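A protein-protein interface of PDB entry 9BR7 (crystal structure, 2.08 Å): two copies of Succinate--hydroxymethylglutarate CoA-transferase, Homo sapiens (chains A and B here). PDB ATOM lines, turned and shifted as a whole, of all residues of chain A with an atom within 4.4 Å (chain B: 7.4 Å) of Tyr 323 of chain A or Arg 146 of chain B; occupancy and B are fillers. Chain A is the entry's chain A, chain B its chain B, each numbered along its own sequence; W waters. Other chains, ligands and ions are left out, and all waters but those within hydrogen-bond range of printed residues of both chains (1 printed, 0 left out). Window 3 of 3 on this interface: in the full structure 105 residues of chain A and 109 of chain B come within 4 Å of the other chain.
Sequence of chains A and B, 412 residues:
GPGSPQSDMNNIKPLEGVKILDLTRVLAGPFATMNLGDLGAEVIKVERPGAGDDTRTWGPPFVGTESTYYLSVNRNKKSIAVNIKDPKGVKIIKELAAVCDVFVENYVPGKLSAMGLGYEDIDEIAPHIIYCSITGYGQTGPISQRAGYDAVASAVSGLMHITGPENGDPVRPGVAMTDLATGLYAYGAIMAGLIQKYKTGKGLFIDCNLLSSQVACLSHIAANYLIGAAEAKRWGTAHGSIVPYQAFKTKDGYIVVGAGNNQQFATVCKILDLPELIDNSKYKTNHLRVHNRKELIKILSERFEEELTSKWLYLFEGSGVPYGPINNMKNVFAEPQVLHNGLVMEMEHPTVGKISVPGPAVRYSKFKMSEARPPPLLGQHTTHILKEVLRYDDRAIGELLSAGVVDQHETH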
ATOM      1  N   VAL A 256       7.962  19.738 -25.832  1.00  0.00           N
ATOM      2  CA  VAL A 256       8.604  20.793 -25.057  1.00  0.00           C
ATOM      3  C   VAL A 256       9.979  21.054 -25.652  1.00  0.00           C
ATOM      4  O   VAL A 256      10.772  20.124 -25.841  1.00  0.00           O
ATOM      5  CB  VAL A 256       8.707  20.404 -23.572  1.00  0.00           C
ATOM      6  CG1 VAL A 256       9.515  21.441 -22.802  1.00  0.00           C
ATOM      7  CG2 VAL A 256       7.321  20.242 -22.967  1.00  0.00           C
ATOM      8  N   VAL A 257      10.258  22.317 -25.964  1.00  0.00           N
ATOM      9  CA  VAL A 257      11.537  22.731 -26.531  1.00  0.00           C
ATOM     10  C   VAL A 257      11.932  24.058 -25.904  1.00  0.00           C
ATOM     11  O   VAL A 257      11.081  24.926 -25.679  1.00  0.00           O
ATOM     12  CB  VAL A 257      11.466  22.852 -28.069  1.00  0.00           C
ATOM     13  CG1 VAL A 257      12.778  23.395 -28.625  1.00  0.00           C
ATOM     14  CG2 VAL A 257      11.123  21.509 -28.698  1.00  0.00           C
ATOM     15  N   LEU A 313      11.119  14.803 -32.717  1.00  0.00           N
ATOM     16  CA  LEU A 313      12.025  14.112 -31.806  1.00  0.00           C
ATOM     17  C   LEU A 313      13.263  13.604 -32.537  1.00  0.00           C
ATOM     18  O   LEU A 313      14.377  13.663 -32.002  1.00  0.00           O
ATOM     19  CB  LEU A 313      11.294  12.960 -31.114  1.00  0.00           C
ATOM     20  CG  LEU A 313      10.173  13.366 -30.155  1.00  0.00           C
ATOM     21  CD1 LEU A 313       9.560  12.142 -29.492  1.00  0.00           C
ATOM     22  CD2 LEU A 313      10.687  14.345 -29.107  1.00  0.00           C
ATOM     23  N   PHE A 316      15.628  16.573 -33.388  1.00  0.00           N
ATOM     24  CA  PHE A 316      16.271  17.182 -32.232  1.00  0.00           C
ATOM     25  C   PHE A 316      17.295  16.275 -31.560  1.00  0.00           C
ATOM     26  O   PHE A 316      17.916  16.697 -30.579  1.00  0.00           O
ATOM     27  CB  PHE A 316      15.217  17.611 -31.207  1.00  0.00           C
ATOM     28  CG  PHE A 316      14.658  18.981 -31.457  1.00  0.00           C
ATOM     29  CD1 PHE A 316      15.309  20.105 -30.975  1.00  0.00           C
ATOM     30  CD2 PHE A 316      13.492  19.147 -32.184  1.00  0.00           C
ATOM     31  CE1 PHE A 316      14.801  21.369 -31.207  1.00  0.00           C
ATOM     32  CE2 PHE A 316      12.980  20.409 -32.421  1.00  0.00           C
ATOM     33  CZ  PHE A 316      13.634  21.522 -31.932  1.00  0.00           C
ATOM     34  N   GLU A 317      17.493  15.054 -32.053  1.00  0.00           N
ATOM     35  CA  GLU A 317      18.500  14.180 -31.464  1.00  0.00           C
ATOM     36  C   GLU A 317      19.865  14.854 -31.534  1.00  0.00           C
ATOM     37  O   GLU A 317      20.277  15.339 -32.592  1.00  0.00           O
ATOM     38  CB  GLU A 317      18.542  12.831 -32.178  1.00  0.00           C
ATOM     39  CG  GLU A 317      17.289  11.990 -32.009  1.00  0.00           C
ATOM     40  CD  GLU A 317      17.397  10.643 -32.699  1.00  0.00           C
ATOM     41  OE1 GLU A 317      18.511  10.296 -33.148  1.00  0.00           O
ATOM     42  OE2 GLU A 317      16.367   9.943 -32.813  1.00  0.00           O
ATOM     43  N   SER A 319      20.738  17.650 -30.427  1.00  0.00           N
ATOM     44  CA  SER A 319      20.710  19.107 -30.481  1.00  0.00           C
ATOM     45  C   SER A 319      21.365  19.720 -29.253  1.00  0.00           C
ATOM     46  O   SER A 319      21.885  20.840 -29.319  1.00  0.00           O
ATOM     47  CB  SER A 319      19.270  19.603 -30.607  1.00  0.00           C
ATOM     48  OG  SER A 319      18.505  19.220 -29.478  1.00  0.00           O
ATOM     49  N   VAL A 321      19.784  20.755 -26.672  1.00  0.00           N
ATOM     50  CA  VAL A 321      18.857  21.697 -26.051  1.00  0.00           C
ATOM     51  C   VAL A 321      17.811  20.915 -25.267  1.00  0.00           C
ATOM     52  O   VAL A 321      17.585  19.729 -25.548  1.00  0.00           O
ATOM     53  CB  VAL A 321      18.189  22.599 -27.101  1.00  0.00           C
ATOM     54  CG1 VAL A 321      19.239  23.293 -27.957  1.00  0.00           C
ATOM     55  CG2 VAL A 321      17.230  21.787 -27.962  1.00  0.00           C
ATOM     56  N   PRO A 322      17.143  21.531 -24.291  1.00  0.00           N
ATOM     57  CA  PRO A 322      16.058  20.840 -23.579  1.00  0.00           C
ATOM     58  C   PRO A 322      14.890  20.576 -24.520  1.00  0.00           C
ATOM     59  O   PRO A 322      14.343  21.501 -25.123  1.00  0.00           O
ATOM     60  CB  PRO A 322      15.678  21.821 -22.463  1.00  0.00           C
ATOM     61  CG  PRO A 322      16.166  23.152 -22.937  1.00  0.00           C
ATOM     62  CD  PRO A 322      17.393  22.880 -23.755  1.00  0.00           C
ATOM     63  N   TYR A 323      14.522  19.304 -24.653  1.00  0.00           N
ATOM     64  CA  TYR A 323      13.393  18.934 -25.494  1.00  0.00           C
ATOM     65  C   TYR A 323      12.868  17.580 -25.043  1.00  0.00           C
ATOM     66  O   TYR A 323      13.634  16.715 -24.608  1.00  0.00           O
ATOM     67  CB  TYR A 323      13.783  18.888 -26.976  1.00  0.00           C
ATOM     68  CG  TYR A 323      14.536  17.637 -27.370  1.00  0.00           C
ATOM     69  CD1 TYR A 323      15.914  17.554 -27.215  1.00  0.00           C
ATOM     70  CD2 TYR A 323      13.869  16.540 -27.901  1.00  0.00           C
ATOM     71  CE1 TYR A 323      16.607  16.412 -27.573  1.00  0.00           C
ATOM     72  CE2 TYR A 323      14.553  15.393 -28.262  1.00  0.00           C
ATOM     73  CZ  TYR A 323      15.922  15.336 -28.096  1.00  0.00           C
ATOM     74  OH  TYR A 323      16.609  14.198 -28.453  1.00  0.00           O
ATOM     75  N   GLY A 324      11.557  17.407 -25.163  1.00  0.00           N
ATOM     76  CA  GLY A 324      10.912  16.168 -24.808  1.00  0.00           C
ATOM     77  C   GLY A 324       9.443  16.177 -25.173  1.00  0.00           C
ATOM     78  O   GLY A 324       8.793  17.227 -25.197  1.00  0.00           O
ATOM     79  N   TYR B 107      25.868  15.659 -12.752  1.00  0.00           N
ATOM     80  CA  TYR B 107      26.321  15.690 -14.131  1.00  0.00           C
ATOM     81  C   TYR B 107      25.701  14.535 -14.908  1.00  0.00           C
ATOM     82  O   TYR B 107      25.183  13.572 -14.334  1.00  0.00           O
ATOM     83  CB  TYR B 107      27.846  15.592 -14.205  1.00  0.00           C
ATOM     84  CG  TYR B 107      28.584  16.804 -13.689  1.00  0.00           C
ATOM     85  CD1 TYR B 107      28.745  17.934 -14.478  1.00  0.00           C
ATOM     86  CD2 TYR B 107      29.126  16.816 -12.412  1.00  0.00           C
ATOM     87  CE1 TYR B 107      29.424  19.042 -14.010  1.00  0.00           C
ATOM     88  CE2 TYR B 107      29.805  17.919 -11.933  1.00  0.00           C
ATOM     89  CZ  TYR B 107      29.951  19.029 -12.736  1.00  0.00           C
ATOM     90  OH  TYR B 107      30.627  20.128 -12.261  1.00  0.00           O
ATOM     91  N   VAL B 108      25.751  14.644 -16.233  1.00  0.00           N
ATOM     92  CA  VAL B 108      25.288  13.522 -17.055  1.00  0.00           C
ATOM     93  C   VAL B 108      26.047  12.266 -16.652  1.00  0.00           C
ATOM     94  O   VAL B 108      27.249  12.350 -16.325  1.00  0.00           O
ATOM     95  CB  VAL B 108      25.478  13.826 -18.549  1.00  0.00           C
ATOM     96  CG1 VAL B 108      25.387  12.549 -19.373  1.00  0.00           C
ATOM     97  CG2 VAL B 108      24.442  14.839 -19.016  1.00  0.00           C
ATOM     98  N   PRO B 109      25.416  11.094 -16.632  1.00  0.00           N
ATOM     99  CA  PRO B 109      26.134   9.881 -16.217  1.00  0.00           C
ATOM    100  C   PRO B 109      27.380   9.672 -17.065  1.00  0.00           C
ATOM    101  O   PRO B 109      27.348   9.795 -18.291  1.00  0.00           O
ATOM    102  CB  PRO B 109      25.103   8.764 -16.426  1.00  0.00           C
ATOM    103  CG  PRO B 109      24.051   9.355 -17.317  1.00  0.00           C
ATOM    104  CD  PRO B 109      24.017  10.812 -16.988  1.00  0.00           C
ATOM    105  N   THR B 135      20.434  12.692 -11.821  1.00  0.00           N
ATOM    106  CA  THR B 135      20.412  12.841 -13.269  1.00  0.00           C
ATOM    107  C   THR B 135      18.977  13.033 -13.754  1.00  0.00           C
ATOM    108  O   THR B 135      18.019  13.020 -12.976  1.00  0.00           O
ATOM    109  CB  THR B 135      21.050  11.630 -13.955  1.00  0.00           C
ATOM    110  OG1 THR B 135      20.336  10.441 -13.587  1.00  0.00           O
ATOM    111  CG2 THR B 135      22.508  11.491 -13.538  1.00  0.00           C
ATOM    112  N   GLY B 136      18.841  13.200 -15.066  1.00  0.00           N
ATOM    113  CA  GLY B 136      17.540  13.377 -15.675  1.00  0.00           C
ATOM    114  C   GLY B 136      16.770  12.080 -15.794  1.00  0.00           C
ATOM    115  O   GLY B 136      15.556  12.050 -15.576  1.00  0.00           O
ATOM    116  N   TYR B 137      17.468  10.995 -16.129  1.00  0.00           N
ATOM    117  CA  TYR B 137      16.797   9.746 -16.448  1.00  0.00           C
ATOM    118  C   TYR B 137      17.426   8.516 -15.807  1.00  0.00           C
ATOM    119  O   TYR B 137      16.948   7.405 -16.062  1.00  0.00           O
ATOM    120  CB  TYR B 137      16.761   9.554 -17.973  1.00  0.00           C
ATOM    121  CG  TYR B 137      16.232  10.760 -18.713  1.00  0.00           C
ATOM    122  CD1 TYR B 137      17.083  11.796 -19.086  1.00  0.00           C
ATOM    123  CD2 TYR B 137      14.884  10.876 -19.022  1.00  0.00           C
ATOM    124  CE1 TYR B 137      16.607  12.905 -19.755  1.00  0.00           C
ATOM    125  CE2 TYR B 137      14.399  11.982 -19.693  1.00  0.00           C
ATOM    126  CZ  TYR B 137      15.263  12.993 -20.057  1.00  0.00           C
ATOM    127  OH  TYR B 137      14.781  14.094 -20.723  1.00  0.00           O
ATOM    128  N   GLY B 138      18.452   8.667 -14.984  1.00  0.00           N
ATOM    129  CA  GLY B 138      19.133   7.540 -14.384  1.00  0.00           C
ATOM    130  C   GLY B 138      20.521   7.334 -14.971  1.00  0.00           C
ATOM    131  O   GLY B 138      20.931   7.976 -15.937  1.00  0.00           O
ATOM    132  N   PRO B 142      18.495   3.648 -22.528  1.00  0.00           N
ATOM    133  CA  PRO B 142      18.642   4.163 -23.901  1.00  0.00           C
ATOM    134  C   PRO B 142      18.811   5.672 -23.974  1.00  0.00           C
ATOM    135  O   PRO B 142      19.560   6.161 -24.829  1.00  0.00           O
ATOM    136  CB  PRO B 142      17.349   3.698 -24.590  1.00  0.00           C
ATOM    137  CG  PRO B 142      16.395   3.392 -23.477  1.00  0.00           C
ATOM    138  CD  PRO B 142      17.234   2.913 -22.337  1.00  0.00           C
ATOM    139  N   ILE B 143      18.137   6.425 -23.111  1.00  0.00           N
ATOM    140  CA  ILE B 143      18.176   7.881 -23.152  1.00  0.00           C
ATOM    141  C   ILE B 143      18.851   8.462 -21.908  1.00  0.00           C
ATOM    142  O   ILE B 143      18.631   9.623 -21.570  1.00  0.00           O
ATOM    143  CB  ILE B 143      16.769   8.468 -23.345  1.00  0.00           C
ATOM    144  CG1 ILE B 143      15.866   8.084 -22.172  1.00  0.00           C
ATOM    145  CG2 ILE B 143      16.165   7.983 -24.653  1.00  0.00           C
ATOM    146  CD1 ILE B 143      14.507   8.748 -22.204  1.00  0.00           C
ATOM    147  N   SER B 144      19.676   7.670 -21.221  1.00  0.00           N
ATOM    148  CA  SER B 144      20.316   8.123 -19.990  1.00  0.00           C
ATOM    149  C   SER B 144      21.359   9.212 -20.214  1.00  0.00           C
ATOM    150  O   SER B 144      21.773   9.854 -19.243  1.00  0.00           O
ATOM    151  CB  SER B 144      20.959   6.935 -19.273  1.00  0.00           C
ATOM    152  OG  SER B 144      21.987   6.358 -20.060  1.00  0.00           O
ATOM    153  N   GLN B 145      21.793   9.443 -21.453  1.00  0.00           N
ATOM    154  CA  GLN B 145      22.814  10.448 -21.722  1.00  0.00           C
ATOM    155  C   GLN B 145      22.255  11.857 -21.879  1.00  0.00           C
ATOM    156  O   GLN B 145      23.039  12.803 -22.005  1.00  0.00           O
ATOM    157  CB  GLN B 145      23.603  10.072 -22.977  1.00  0.00           C
ATOM    158  CG  GLN B 145      24.680   9.025 -22.743  1.00  0.00           C
ATOM    159  CD  GLN B 145      25.764   9.509 -21.795  1.00  0.00           C
ATOM    160  OE1 GLN B 145      26.460  10.484 -22.081  1.00  0.00           O
ATOM    161  NE2 GLN B 145      25.912   8.830 -20.664  1.00  0.00           N
ATOM    162  N   ARG B 146      20.935  12.026 -21.873  1.00  0.00           N
ATOM    163  CA  ARG B 146      20.346  13.354 -21.966  1.00  0.00           C
ATOM    164  C   ARG B 146      20.432  14.080 -20.630  1.00  0.00           C
ATOM    165  O   ARG B 146      20.271  13.477 -19.565  1.00  0.00           O
ATOM    166  CB  ARG B 146      18.887  13.260 -22.413  1.00  0.00           C
ATOM    167  CG  ARG B 146      18.707  12.673 -23.798  1.00  0.00           C
ATOM    168  CD  ARG B 146      17.244  12.637 -24.196  1.00  0.00           C
ATOM    169  NE  ARG B 146      17.052  11.958 -25.470  1.00  0.00           N
ATOM    170  CZ  ARG B 146      15.870  11.643 -25.980  1.00  0.00           C
ATOM    171  NH1 ARG B 146      14.746  11.928 -25.343  1.00  0.00           N
ATOM    172  NH2 ARG B 146      15.814  11.028 -27.157  1.00  0.00           N
ATOM    173  N   ALA B 147      20.685  15.385 -20.693  1.00  0.00           N
ATOM    174  CA  ALA B 147      20.719  16.198 -19.489  1.00  0.00           C
ATOM    175  C   ALA B 147      19.312  16.355 -18.919  1.00  0.00           C
ATOM    176  O   ALA B 147      18.316  16.325 -19.644  1.00  0.00           O
ATOM    177  CB  ALA B 147      21.326  17.570 -19.782  1.00  0.00           C
ATOM    178  N   GLY B 148      19.240  16.522 -17.599  1.00  0.00           N
ATOM    179  CA  GLY B 148      17.965  16.618 -16.918  1.00  0.00           C
ATOM    180  C   GLY B 148      17.433  18.038 -16.893  1.00  0.00           C
ATOM    181  O   GLY B 148      18.171  18.984 -16.605  1.00  0.00           O
ATOM    182  N   TYR B 149      16.146  18.179 -17.204  1.00  0.00           N
ATOM    183  CA  TYR B 149      15.447  19.452 -17.121  1.00  0.00           C
ATOM    184  C   TYR B 149      14.070  19.200 -16.532  1.00  0.00           C
ATOM    185  O   TYR B 149      13.389  18.247 -16.921  1.00  0.00           O
ATOM    186  CB  TYR B 149      15.294  20.122 -18.495  1.00  0.00           C
ATOM    187  CG  TYR B 149      16.582  20.396 -19.240  1.00  0.00           C
ATOM    188  CD1 TYR B 149      17.117  19.455 -20.109  1.00  0.00           C
ATOM    189  CD2 TYR B 149      17.245  21.608 -19.100  1.00  0.00           C
ATOM    190  CE1 TYR B 149      18.285  19.705 -20.806  1.00  0.00           C
ATOM    191  CE2 TYR B 149      18.416  21.869 -19.795  1.00  0.00           C
ATOM    192  CZ  TYR B 149      18.931  20.913 -20.645  1.00  0.00           C
ATOM    193  OH  TYR B 149      20.091  21.163 -21.338  1.00  0.00           O
ATOM    194  N   ALA B 151      11.177  20.847 -16.814  1.00  0.00           N
ATOM    195  CA  ALA B 151      10.062  20.940 -17.752  1.00  0.00           C
ATOM    196  C   ALA B 151      10.020  19.732 -18.679  1.00  0.00           C
ATOM    197  O   ALA B 151       8.939  19.238 -19.018  1.00  0.00           O
ATOM    198  CB  ALA B 151      10.157  22.234 -18.561  1.00  0.00           C
ATOM    199  N   VAL B 152      11.186  19.246 -19.102  1.00  0.00           N
ATOM    200  CA  VAL B 152      11.223  18.068 -19.963  1.00  0.00           C
ATOM    201  C   VAL B 152      10.793  16.829 -19.187  1.00  0.00           C
ATOM    202  O   VAL B 152      10.015  16.008 -19.686  1.00  0.00           O
ATOM    203  CB  VAL B 152      12.623  17.897 -20.578  1.00  0.00           C
ATOM    204  CG1 VAL B 152      12.677  16.638 -21.426  1.00  0.00           C
ATOM    205  CG2 VAL B 152      12.984  19.117 -21.411  1.00  0.00           C
ATOM    206  N   ALA B 153      11.293  16.672 -17.959  1.00  0.00           N
ATOM    207  CA  ALA B 153      10.941  15.504 -17.160  1.00  0.00           C
ATOM    208  C   ALA B 153       9.438  15.440 -16.910  1.00  0.00           C
ATOM    209  O   ALA B 153       8.817  14.381 -17.053  1.00  0.00           O
ATOM    210  CB  ALA B 153      11.710  15.521 -15.838  1.00  0.00           C
ATOM    211  N   ALA B 155       7.184  16.569 -18.738  1.00  0.00           N
ATOM    212  CA  ALA B 155       6.520  16.235 -19.993  1.00  0.00           C
ATOM    213  C   ALA B 155       6.642  14.747 -20.298  1.00  0.00           C
ATOM    214  O   ALA B 155       5.647  14.084 -20.611  1.00  0.00           O
ATOM    215  CB  ALA B 155       7.100  17.069 -21.138  1.00  0.00           C
ATOM    216  N   VAL B 156       7.861  14.210 -20.212  1.00  0.00           N
ATOM    217  CA  VAL B 156       8.096  12.804 -20.526  1.00  0.00           C
ATOM    218  C   VAL B 156       7.464  11.889 -19.483  1.00  0.00           C
ATOM    219  O   VAL B 156       7.050  10.767 -19.803  1.00  0.00           O
ATOM    220  CB  VAL B 156       9.608  12.545 -20.651  1.00  0.00           C
ATOM    221  CG1 VAL B 156       9.894  11.051 -20.653  1.00  0.00           C
ATOM    222  CG2 VAL B 156      10.162  13.207 -21.910  1.00  0.00           C
HETATM  223  O   HOH W   1      15.115  12.292 -29.641  1.00  0.00           O
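Water W1 lies within hydrogen-bond range of OH of Tyr 323 of chain A, O of Leu 313 of chain A and NH2 of Arg 146 of chain B.
No position is printed for both chains.
Of the 6 pairs that touch across the chains among the printed residues, none has its exchanged pair printed and touching as well.
Among the printed residues, pairs that only touch across the chains: Val 256 of chain A with Ala 155 of chain B (3.7 Å), Pro 322 of chain A with Tyr 149 of chain B (3.6 Å), Pro 322 of chain A with Val 152 of chain B (3.9 Å), Tyr 323 of chain A with Arg 146 of chain B (3.5 Å), Tyr 323 of chain A with Val 152 of chain B (3.3 Å) and Gly 324 of chain A with Val 152 of chain B (3.8 Å).
Printed residues of chain A that touch a printed residue of chain B: Val 256, Pro 322, Tyr 323 and Gly 324.
Among the printed residues, no Asp or Glu carboxylate lies within 4 Å of a Lys or Arg side-chain nitrogen of the other chain.
The backbone NH (N) of Val 256 of chain A sits at hydrogen-bond distance from the backbone carbonyl oxygen (O) of Gly 324 of chain A, at 2.7 Å.
Phe 316 of chain A touches none of the printed residues of chain B.
Printed residues of chain B within 4 Å of Pro 322 of chain A: Tyr 149 (3.6 Å) and Val 152 (3.9 Å).
Of the printed residues of chain B, Tyr 323 of chain A touches Arg 146 (3.5 Å) and Val 152 (3.3 Å).
Tyr 137 of chain B touches none of the printed residues of chain A.
Of chain A, only Tyr 323 comes within 4 Å of Arg 146 of chain B.
Of the printed residues of chain A, Tyr 149 of chain B touches Pro 322 (3.6 Å).
Of the printed residues of chain A, Val 152 of chain B touches Pro 322, Tyr 323 and Gly 324.
Of the printed residues of chain A, Ala 155 of chain B touches Val 256 (3.7 Å).
The nearest residue of chain B that does not touch Tyr 323 of chain A is Tyr 137 of chain B (4.8 Å).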
